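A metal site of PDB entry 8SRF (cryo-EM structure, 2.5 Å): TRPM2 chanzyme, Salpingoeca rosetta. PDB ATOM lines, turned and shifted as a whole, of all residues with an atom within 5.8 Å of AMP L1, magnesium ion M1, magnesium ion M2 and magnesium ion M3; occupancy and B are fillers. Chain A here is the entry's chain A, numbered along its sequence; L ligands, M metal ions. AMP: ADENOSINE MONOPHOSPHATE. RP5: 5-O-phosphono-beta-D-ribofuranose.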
ATOM      1  N   LYS A1225       5.780  21.528 -31.371  1.00  0.00           N
ATOM      2  CA  LYS A1225       5.172  22.516 -32.315  1.00  0.00           C
ATOM      3  C   LYS A1225       6.172  23.542 -32.902  1.00  0.00           C
ATOM      4  O   LYS A1225       5.788  24.645 -33.285  1.00  0.00           O
ATOM      5  CB  LYS A1225       3.981  23.231 -31.665  1.00  0.00           C
ATOM      6  CG  LYS A1225       2.844  22.311 -31.272  1.00  0.00           C
ATOM      7  CD  LYS A1225       1.556  23.078 -31.063  1.00  0.00           C
ATOM      8  CE  LYS A1225       1.584  23.870 -29.768  1.00  0.00           C
ATOM      9  NZ  LYS A1225       0.301  24.597 -29.518  1.00  0.00           N
ATOM     10  N   TRP A1264      -0.869  38.427 -23.762  1.00  0.00           N
ATOM     11  CA  TRP A1264      -0.372  37.652 -22.627  1.00  0.00           C
ATOM     12  C   TRP A1264       1.128  37.403 -22.690  1.00  0.00           C
ATOM     13  O   TRP A1264       1.647  36.632 -21.879  1.00  0.00           O
ATOM     14  CB  TRP A1264      -1.076  36.287 -22.565  1.00  0.00           C
ATOM     15  CG  TRP A1264      -1.260  35.588 -23.898  1.00  0.00           C
ATOM     16  CD1 TRP A1264      -2.347  35.671 -24.725  1.00  0.00           C
ATOM     17  CD2 TRP A1264      -0.320  34.743 -24.574  1.00  0.00           C
ATOM     18  NE1 TRP A1264      -2.160  34.917 -25.846  1.00  0.00           N
ATOM     19  CE2 TRP A1264      -0.920  34.335 -25.782  1.00  0.00           C
ATOM     20  CE3 TRP A1264       0.974  34.279 -24.265  1.00  0.00           C
ATOM     21  CZ2 TRP A1264      -0.267  33.490 -26.695  1.00  0.00           C
ATOM     22  CZ3 TRP A1264       1.619  33.432 -25.160  1.00  0.00           C
ATOM     23  CH2 TRP A1264       0.987  33.050 -26.367  1.00  0.00           C
ATOM     24  N   LEU A1319       7.769  28.454 -26.516  1.00  0.00           N
ATOM     25  CA  LEU A1319       6.319  28.568 -26.617  1.00  0.00           C
ATOM     26  C   LEU A1319       5.691  29.305 -25.440  1.00  0.00           C
ATOM     27  O   LEU A1319       4.483  29.580 -25.480  1.00  0.00           O
ATOM     28  CB  LEU A1319       5.670  27.188 -26.688  1.00  0.00           C
ATOM     29  CG  LEU A1319       5.463  26.494 -28.020  1.00  0.00           C
ATOM     30  CD1 LEU A1319       5.146  25.042 -27.765  1.00  0.00           C
ATOM     31  CD2 LEU A1319       4.297  27.148 -28.719  1.00  0.00           C
ATOM     32  N   LEU A1320       6.468  29.627 -24.419  1.00  0.00           N
ATOM     33  CA  LEU A1320       5.947  30.262 -23.218  1.00  0.00           C
ATOM     34  C   LEU A1320       6.003  31.771 -23.387  1.00  0.00           C
ATOM     35  O   LEU A1320       6.994  32.313 -23.873  1.00  0.00           O
ATOM     36  CB  LEU A1320       6.766  29.816 -22.014  1.00  0.00           C
ATOM     37  CG  LEU A1320       6.730  28.297 -21.804  1.00  0.00           C
ATOM     38  CD1 LEU A1320       7.535  27.936 -20.605  1.00  0.00           C
ATOM     39  CD2 LEU A1320       5.322  27.730 -21.675  1.00  0.00           C
ATOM     40  N   GLY A1321       4.927  32.451 -22.979  1.00  0.00           N
ATOM     41  CA  GLY A1321       4.813  33.869 -23.265  1.00  0.00           C
ATOM     42  C   GLY A1321       5.497  34.772 -22.266  1.00  0.00           C
ATOM     43  O   GLY A1321       5.834  35.908 -22.616  1.00  0.00           O
ATOM     44  N   LYS A1322       5.745  34.291 -21.060  1.00  0.00           N
ATOM     45  CA  LYS A1322       6.288  35.119 -19.995  1.00  0.00           C
ATOM     46  C   LYS A1322       7.700  34.672 -19.638  1.00  0.00           C
ATOM     47  O   LYS A1322       7.968  33.465 -19.583  1.00  0.00           O
ATOM     48  CB  LYS A1322       5.395  35.074 -18.761  1.00  0.00           C
ATOM     49  CG  LYS A1322       3.980  35.570 -19.000  1.00  0.00           C
ATOM     50  CD  LYS A1322       3.156  35.533 -17.732  1.00  0.00           C
ATOM     51  CE  LYS A1322       1.679  35.698 -18.039  1.00  0.00           C
ATOM     52  NZ  LYS A1322       1.415  36.935 -18.826  1.00  0.00           N
ATOM     53  N   ASN A1326       6.208  30.961 -15.513  1.00  0.00           N
ATOM     54  CA  ASN A1326       4.858  30.939 -16.034  1.00  0.00           C
ATOM     55  C   ASN A1326       3.985  30.221 -15.016  1.00  0.00           C
ATOM     56  O   ASN A1326       4.144  29.015 -14.800  1.00  0.00           O
ATOM     57  CB  ASN A1326       4.815  30.268 -17.397  1.00  0.00           C
ATOM     58  CG  ASN A1326       5.315  31.162 -18.510  1.00  0.00           C
ATOM     59  OD1 ASN A1326       4.532  31.769 -19.237  1.00  0.00           O
ATOM     60  ND2 ASN A1326       6.632  31.265 -18.629  1.00  0.00           N
ATOM     61  N   ILE A1358      -8.686  15.537 -19.226  1.00  0.00           N
ATOM     62  CA  ILE A1358      -8.889  16.044 -20.575  1.00  0.00           C
ATOM     63  C   ILE A1358      -7.778  15.549 -21.508  1.00  0.00           C
ATOM     64  O   ILE A1358      -6.680  15.186 -21.087  1.00  0.00           O
ATOM     65  CB  ILE A1358      -8.980  17.588 -20.585  1.00  0.00           C
ATOM     66  CG1 ILE A1358      -7.666  18.227 -20.110  1.00  0.00           C
ATOM     67  CG2 ILE A1358     -10.185  18.058 -19.801  1.00  0.00           C
ATOM     68  CD1 ILE A1358      -7.364  19.545 -20.638  1.00  0.00           C
ATOM     69  N   ARG A1360      -5.521  16.648 -24.371  1.00  0.00           N
ATOM     70  CA  ARG A1360      -4.982  17.904 -24.885  1.00  0.00           C
ATOM     71  C   ARG A1360      -5.032  17.958 -26.409  1.00  0.00           C
ATOM     72  O   ARG A1360      -4.910  16.933 -27.088  1.00  0.00           O
ATOM     73  CB  ARG A1360      -3.555  18.107 -24.401  1.00  0.00           C
ATOM     74  CG  ARG A1360      -3.421  18.118 -22.894  1.00  0.00           C
ATOM     75  CD  ARG A1360      -1.987  18.346 -22.491  1.00  0.00           C
ATOM     76  NE  ARG A1360      -1.404  19.514 -23.144  1.00  0.00           N
ATOM     77  CZ  ARG A1360      -1.482  20.760 -22.678  1.00  0.00           C
ATOM     78  NH1 ARG A1360      -2.118  21.039 -21.553  1.00  0.00           N
ATOM     79  NH2 ARG A1360      -0.910  21.737 -23.353  1.00  0.00           N
ATOM     80  N   GLY A1370      -6.351  22.795 -16.748  1.00  0.00           N
ATOM     81  CA  GLY A1370      -5.643  23.911 -16.153  1.00  0.00           C
ATOM     82  C   GLY A1370      -5.040  24.755 -17.247  1.00  0.00           C
ATOM     83  O   GLY A1370      -5.079  24.420 -18.434  1.00  0.00           O
ATOM     84  N   GLY A1371      -4.458  25.866 -16.813  1.00  0.00           N
ATOM     85  CA  GLY A1371      -3.893  26.770 -17.782  1.00  0.00           C
ATOM     86  C   GLY A1371      -3.104  27.862 -17.108  1.00  0.00           C
ATOM     87  O   GLY A1371      -3.006  27.909 -15.870  1.00  0.00           O
ATOM     88  N   PHE A1372      -2.456  28.672 -17.951  1.00  0.00           N
ATOM     89  CA  PHE A1372      -1.597  29.751 -17.491  1.00  0.00           C
ATOM     90  C   PHE A1372      -2.393  30.864 -16.829  1.00  0.00           C
ATOM     91  O   PHE A1372      -3.513  31.181 -17.234  1.00  0.00           O
ATOM     92  CB  PHE A1372      -0.773  30.283 -18.662  1.00  0.00           C
ATOM     93  CG  PHE A1372       0.182  29.280 -19.199  1.00  0.00           C
ATOM     94  CD1 PHE A1372       1.335  28.942 -18.468  1.00  0.00           C
ATOM     95  CD2 PHE A1372      -0.095  28.616 -20.403  1.00  0.00           C
ATOM     96  CE1 PHE A1372       2.240  27.994 -18.953  1.00  0.00           C
ATOM     97  CE2 PHE A1372       0.797  27.648 -20.909  1.00  0.00           C
ATOM     98  CZ  PHE A1372       1.959  27.347 -20.180  1.00  0.00           C
ATOM     99  N   VAL A1373      -1.827  31.437 -15.769  1.00  0.00           N
ATOM    100  CA  VAL A1373      -2.458  32.534 -15.042  1.00  0.00           C
ATOM    101  C   VAL A1373      -2.375  33.825 -15.835  1.00  0.00           C
ATOM    102  O   VAL A1373      -1.288  34.264 -16.224  1.00  0.00           O
ATOM    103  CB  VAL A1373      -1.836  32.679 -13.641  1.00  0.00           C
ATOM    104  CG1 VAL A1373      -2.197  34.001 -12.964  1.00  0.00           C
ATOM    105  CG2 VAL A1373      -2.221  31.505 -12.762  1.00  0.00           C
ATOM    106  N   ASP A1374      -3.539  34.405 -16.142  1.00  0.00           N
ATOM    107  CA  ASP A1374      -3.649  35.649 -16.889  1.00  0.00           C
ATOM    108  C   ASP A1374      -3.218  36.840 -16.012  1.00  0.00           C
ATOM    109  O   ASP A1374      -3.096  36.734 -14.786  1.00  0.00           O
ATOM    110  CB  ASP A1374      -5.079  35.846 -17.381  1.00  0.00           C
ATOM    111  CG  ASP A1374      -5.368  35.075 -18.653  1.00  0.00           C
ATOM    112  OD1 ASP A1374      -4.401  34.614 -19.302  1.00  0.00           O
ATOM    113  OD2 ASP A1374      -6.554  34.923 -19.004  1.00  0.00           O
ATOM    114  N   ARG A1385     -12.107  29.258 -14.120  1.00  0.00           N
ATOM    115  CA  ARG A1385     -12.274  29.654 -15.524  1.00  0.00           C
ATOM    116  C   ARG A1385     -11.736  28.615 -16.499  1.00  0.00           C
ATOM    117  O   ARG A1385     -12.410  28.304 -17.492  1.00  0.00           O
ATOM    118  CB  ARG A1385     -11.595  31.013 -15.744  1.00  0.00           C
ATOM    119  CG  ARG A1385     -11.755  31.588 -17.152  1.00  0.00           C
ATOM    120  CD  ARG A1385     -10.984  32.890 -17.303  1.00  0.00           C
ATOM    121  NE  ARG A1385      -9.636  32.841 -16.727  1.00  0.00           N
ATOM    122  CZ  ARG A1385      -8.564  32.354 -17.331  1.00  0.00           C
ATOM    123  NH1 ARG A1385      -8.616  31.837 -18.551  1.00  0.00           N
ATOM    124  NH2 ARG A1385      -7.398  32.386 -16.705  1.00  0.00           N
ATOM    125  N   GLU A1386     -10.534  28.063 -16.225  1.00  0.00           N
ATOM    126  CA  GLU A1386      -9.930  27.005 -17.060  1.00  0.00           C
ATOM    127  C   GLU A1386     -10.704  25.706 -16.987  1.00  0.00           C
ATOM    128  O   GLU A1386     -10.706  24.951 -17.974  1.00  0.00           O
ATOM    129  CB  GLU A1386      -8.443  26.796 -16.787  1.00  0.00           C
ATOM    130  CG  GLU A1386      -7.479  27.926 -17.253  1.00  0.00           C
ATOM    131  CD  GLU A1386      -7.606  28.340 -18.726  1.00  0.00           C
ATOM    132  OE1 GLU A1386      -7.744  27.470 -19.605  1.00  0.00           O
ATOM    133  OE2 GLU A1386      -7.546  29.561 -18.992  1.00  0.00           O
ATOM    134  N   GLU A1389     -13.847  26.365 -19.061  1.00  0.00           N
ATOM    135  CA  GLU A1389     -13.498  26.428 -20.483  1.00  0.00           C
ATOM    136  C   GLU A1389     -13.108  25.077 -21.073  1.00  0.00           C
ATOM    137  O   GLU A1389     -13.491  24.753 -22.198  1.00  0.00           O
ATOM    138  CB  GLU A1389     -12.396  27.459 -20.742  1.00  0.00           C
ATOM    139  CG  GLU A1389     -12.886  28.904 -20.767  1.00  0.00           C
ATOM    140  CD  GLU A1389     -11.746  29.901 -20.711  1.00  0.00           C
ATOM    141  OE1 GLU A1389     -10.572  29.475 -20.677  1.00  0.00           O
ATOM    142  OE2 GLU A1389     -12.023  31.116 -20.714  1.00  0.00           O
ATOM    143  N   GLU A1390     -12.297  24.294 -20.349  1.00  0.00           N
ATOM    144  CA  GLU A1390     -11.737  23.065 -20.906  1.00  0.00           C
ATOM    145  C   GLU A1390     -12.598  21.838 -20.652  1.00  0.00           C
ATOM    146  O   GLU A1390     -12.942  21.127 -21.616  1.00  0.00           O
ATOM    147  CB  GLU A1390     -10.324  22.882 -20.364  1.00  0.00           C
ATOM    148  CG  GLU A1390      -9.363  23.948 -20.886  1.00  0.00           C
ATOM    149  CD  GLU A1390      -7.955  23.802 -20.351  1.00  0.00           C
ATOM    150  OE1 GLU A1390      -7.659  22.784 -19.706  1.00  0.00           O
ATOM    151  OE2 GLU A1390      -7.144  24.709 -20.588  1.00  0.00           O
ATOM    152  N   ARG A1428       7.945  22.022 -22.872  1.00  0.00           N
ATOM    153  CA  ARG A1428       8.127  23.351 -23.444  1.00  0.00           C
ATOM    154  C   ARG A1428       9.030  24.261 -22.610  1.00  0.00           C
ATOM    155  O   ARG A1428       9.183  25.422 -22.986  1.00  0.00           O
ATOM    156  CB  ARG A1428       6.791  24.081 -23.610  1.00  0.00           C
ATOM    157  CG  ARG A1428       5.751  23.341 -24.395  1.00  0.00           C
ATOM    158  CD  ARG A1428       4.389  23.956 -24.155  1.00  0.00           C
ATOM    159  NE  ARG A1428       3.908  23.664 -22.808  1.00  0.00           N
ATOM    160  CZ  ARG A1428       2.730  24.030 -22.339  1.00  0.00           C
ATOM    161  NH1 ARG A1428       1.882  24.727 -23.083  1.00  0.00           N
ATOM    162  NH2 ARG A1428       2.393  23.703 -21.096  1.00  0.00           N
ATOM    163  N   ASP A1459     -12.471  24.459 -25.870  1.00  0.00           N
ATOM    164  CA  ASP A1459     -11.292  25.364 -25.989  1.00  0.00           C
ATOM    165  C   ASP A1459     -10.088  24.531 -26.415  1.00  0.00           C
ATOM    166  O   ASP A1459     -10.112  23.974 -27.528  1.00  0.00           O
ATOM    167  CB  ASP A1459     -11.149  26.172 -24.692  1.00  0.00           C
ATOM    168  CG  ASP A1459     -10.213  27.363 -24.838  1.00  0.00           C
ATOM    169  OD1 ASP A1459      -9.962  27.780 -25.985  1.00  0.00           O
ATOM    170  OD2 ASP A1459      -9.724  27.878 -23.812  1.00  0.00           O
ATOM    171  N   ASP A1460      -9.030  24.412 -25.607  1.00  0.00           N
ATOM    172  CA  ASP A1460      -7.833  23.673 -25.989  1.00  0.00           C
ATOM    173  C   ASP A1460      -7.836  22.243 -25.425  1.00  0.00           C
ATOM    174  O   ASP A1460      -6.770  21.683 -25.160  1.00  0.00           O
ATOM    175  CB  ASP A1460      -6.587  24.462 -25.557  1.00  0.00           C
ATOM    176  CG  ASP A1460      -6.510  24.662 -24.049  1.00  0.00           C
ATOM    177  OD1 ASP A1460      -7.362  25.393 -23.504  1.00  0.00           O
ATOM    178  OD2 ASP A1460      -5.598  24.096 -23.411  1.00  0.00           O
HETATM  179  P   AMP L   1      -4.935  28.050 -21.602  1.00  0.00           P
HETATM  180  O1P AMP L   1      -6.110  28.202 -22.528  1.00  0.00           O
HETATM  181  O2P AMP L   1      -4.911  26.634 -21.080  1.00  0.00           O
HETATM  182  O3P AMP L   1      -4.966  29.180 -20.608  1.00  0.00           O
HETATM  183  O5' AMP L   1      -3.606  28.204 -22.456  1.00  0.00           O
HETATM  184  C5' AMP L   1      -3.559  27.787 -23.805  1.00  0.00           C
HETATM  185  C4' AMP L   1      -3.217  28.939 -24.708  1.00  0.00           C
HETATM  186  O4' AMP L   1      -3.305  30.179 -23.958  1.00  0.00           O
HETATM  187  C3' AMP L   1      -1.804  28.965 -25.273  1.00  0.00           C
HETATM  188  O3' AMP L   1      -1.646  28.100 -26.380  1.00  0.00           O
HETATM  189  C2' AMP L   1      -1.607  30.431 -25.605  1.00  0.00           C
HETATM  190  O2' AMP L   1      -2.258  30.769 -26.813  1.00  0.00           O
HETATM  191  C1' AMP L   1      -2.354  31.104 -24.439  1.00  0.00           C
HETATM  192  N9  AMP L   1      -1.506  31.547 -23.310  1.00  0.00           N
HETATM  193  C8  AMP L   1      -2.004  32.374 -22.393  1.00  0.00           C
HETATM  194  N7  AMP L   1      -1.079  32.639 -21.466  1.00  0.00           N
HETATM  195  C5  AMP L   1       0.020  31.959 -21.808  1.00  0.00           C
HETATM  196  C6  AMP L   1       1.257  31.864 -21.212  1.00  0.00           C
HETATM  197  N6  AMP L   1       1.827  32.457 -20.014  1.00  0.00           N
HETATM  198  N1  AMP L   1       2.223  31.115 -21.717  1.00  0.00           N
HETATM  199  C2  AMP L   1       2.026  30.407 -22.856  1.00  0.00           C
HETATM  200  N3  AMP L   1       0.803  30.508 -23.433  1.00  0.00           N
HETATM  201  C4  AMP L   1      -0.219  31.268 -22.942  1.00  0.00           C
HETATM  202  C1  RP5 L   2       1.454  21.909 -17.278  1.00  0.00           C
HETATM  203  O4  RP5 L   2       1.133  22.574 -18.581  1.00  0.00           O
HETATM  204  C2  RP5 L   2       0.576  22.744 -16.238  1.00  0.00           C
HETATM  205  O2  RP5 L   2       0.349  21.932 -14.995  1.00  0.00           O
HETATM  206  C3  RP5 L   2      -0.479  22.926 -16.857  1.00  0.00           C
HETATM  207  O3  RP5 L   2      -1.436  21.831 -16.572  1.00  0.00           O
HETATM  208  C4  RP5 L   2      -0.121  22.906 -18.478  1.00  0.00           C
HETATM  209  C5  RP5 L   2      -0.359  24.269 -19.043  1.00  0.00           C
HETATM  210  O5  RP5 L   2      -1.671  24.315 -19.514  1.00  0.00           O
HETATM  211  P'  RP5 L   2      -1.890  24.446 -21.128  1.00  0.00           P
HETATM  212  O1X RP5 L   2      -3.170  23.765 -21.526  1.00  0.00           O
HETATM  213  O2X RP5 L   2      -0.735  23.801 -21.851  1.00  0.00           O
HETATM  214  O3X RP5 L   2      -1.955  25.904 -21.485  1.00  0.00           O
HETATM  215  O1  RP5 L   2       2.689  22.029 -16.997  1.00  0.00           O
HETATM  216 MG    MG M   1      -7.087  26.643 -21.463  1.00  0.00          MG
HETATM  217 MG    MG M   2      -5.128  24.516 -21.225  1.00  0.00          MG
HETATM  218 MG    MG M   3      -6.238  30.897 -20.694  1.00  0.00          MG
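N of Gly 1370 sits at hydrogen-bond distance from OE1 of Glu 1390 (3.2 Å). The guanidinium group (NH1) of Arg 1385 sits close to the side-chain carboxylate (OE2) of Glu 1386 (2.6 Å). The backbone carbonyl oxygen of Lys 1322 is in hydrogen-bond range of the side-chain amide nitrogen of Asn 1326. OD2 of Asp 1374 is in salt-bridge range of NH2 of Arg 1385 (3.5 Å). NH1 of Arg 1385 is in salt-bridge range of OE1 of Glu 1389, at 3.7 Å. The side-chain amino group (NZ) of Lys 1322 is in hydrogen-bond range of the backbone carbonyl oxygen (O) of Trp 1264.
The nearest printed residue that does not touch magnesium ion M2 is Glu 1386 (4.3 Å).
Magnesium ion M3 is bound by O3P of AMP L1 (2.1 Å) and OE2 of Glu 1386 (2.5 Å).
OE2 of Glu 1390 is bound to magnesium ion M1, 2.1 Å away. O1P of AMP L1 is bound to magnesium ion M1, 2.1 Å away. OE1 of Glu 1386 binds magnesium ion M1, at 2.1 Å. O2P of AMP L1 binds magnesium ion M1, 2.2 Å away. Magnesium ion M1 is bound by OD1 of Asp 1460 (2.4 Å).
Magnesium ion M2 is bound by O1X of RP5 L2, OE2 of Glu 1390, O2P of AMP L1 and OD2 of Asp 1460. Slightly farther from magnesium ion M2 lies the backbone carbonyl oxygen (O) of Gly 1370 (2.8 Å).
Merely in contact with magnesium ion M1: Asp 1459. Of the 21 residues printed, 4 come within 4 Å of magnesium ion M1.
Residues that only touch magnesium ion M3: Arg 1385. Two residues have an atom within 4 Å of magnesium ion M3: Arg 1385 and Glu 1386. The nearest printed residue that does not touch magnesium ion M3 is Asp 1374 (4.4 Å).
Merely in contact with AMP L1: Trp 1264 (3.4 Å), Leu 1319 (3.7 Å), Leu 1320 (3.9 Å), Lys 1322 (3.8 Å), Gly 1371 (3.5 Å), Phe 1372 (3.4 Å) and Asp 1459 (3.8 Å). Hydrophobic or aromatic side chains that line AMP L1: Trp 1264 and Phe 1372. Of the 21 residues printed, 13 come within 4 Å of AMP L1. The nearest printed residue that does not touch AMP L1 is Asp 1374 (4.4 Å).
The side-chain amide oxygen (OD1) of Asn 1326 lies within hydrogen-bond range of a nitrogen (N6) of AMP L1. N of Gly 1321 lies within hydrogen-bond range of N1 of AMP L1 (3.3 Å). The guanidinium group (NH2) of Arg 1360 lies within salt-bridge range of an oxygen (O2X) of RP5 L2 (2.6 Å). NH1 of Arg 1428 lies within salt-bridge range of O2X of RP5 L2, 3.0 Å away.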
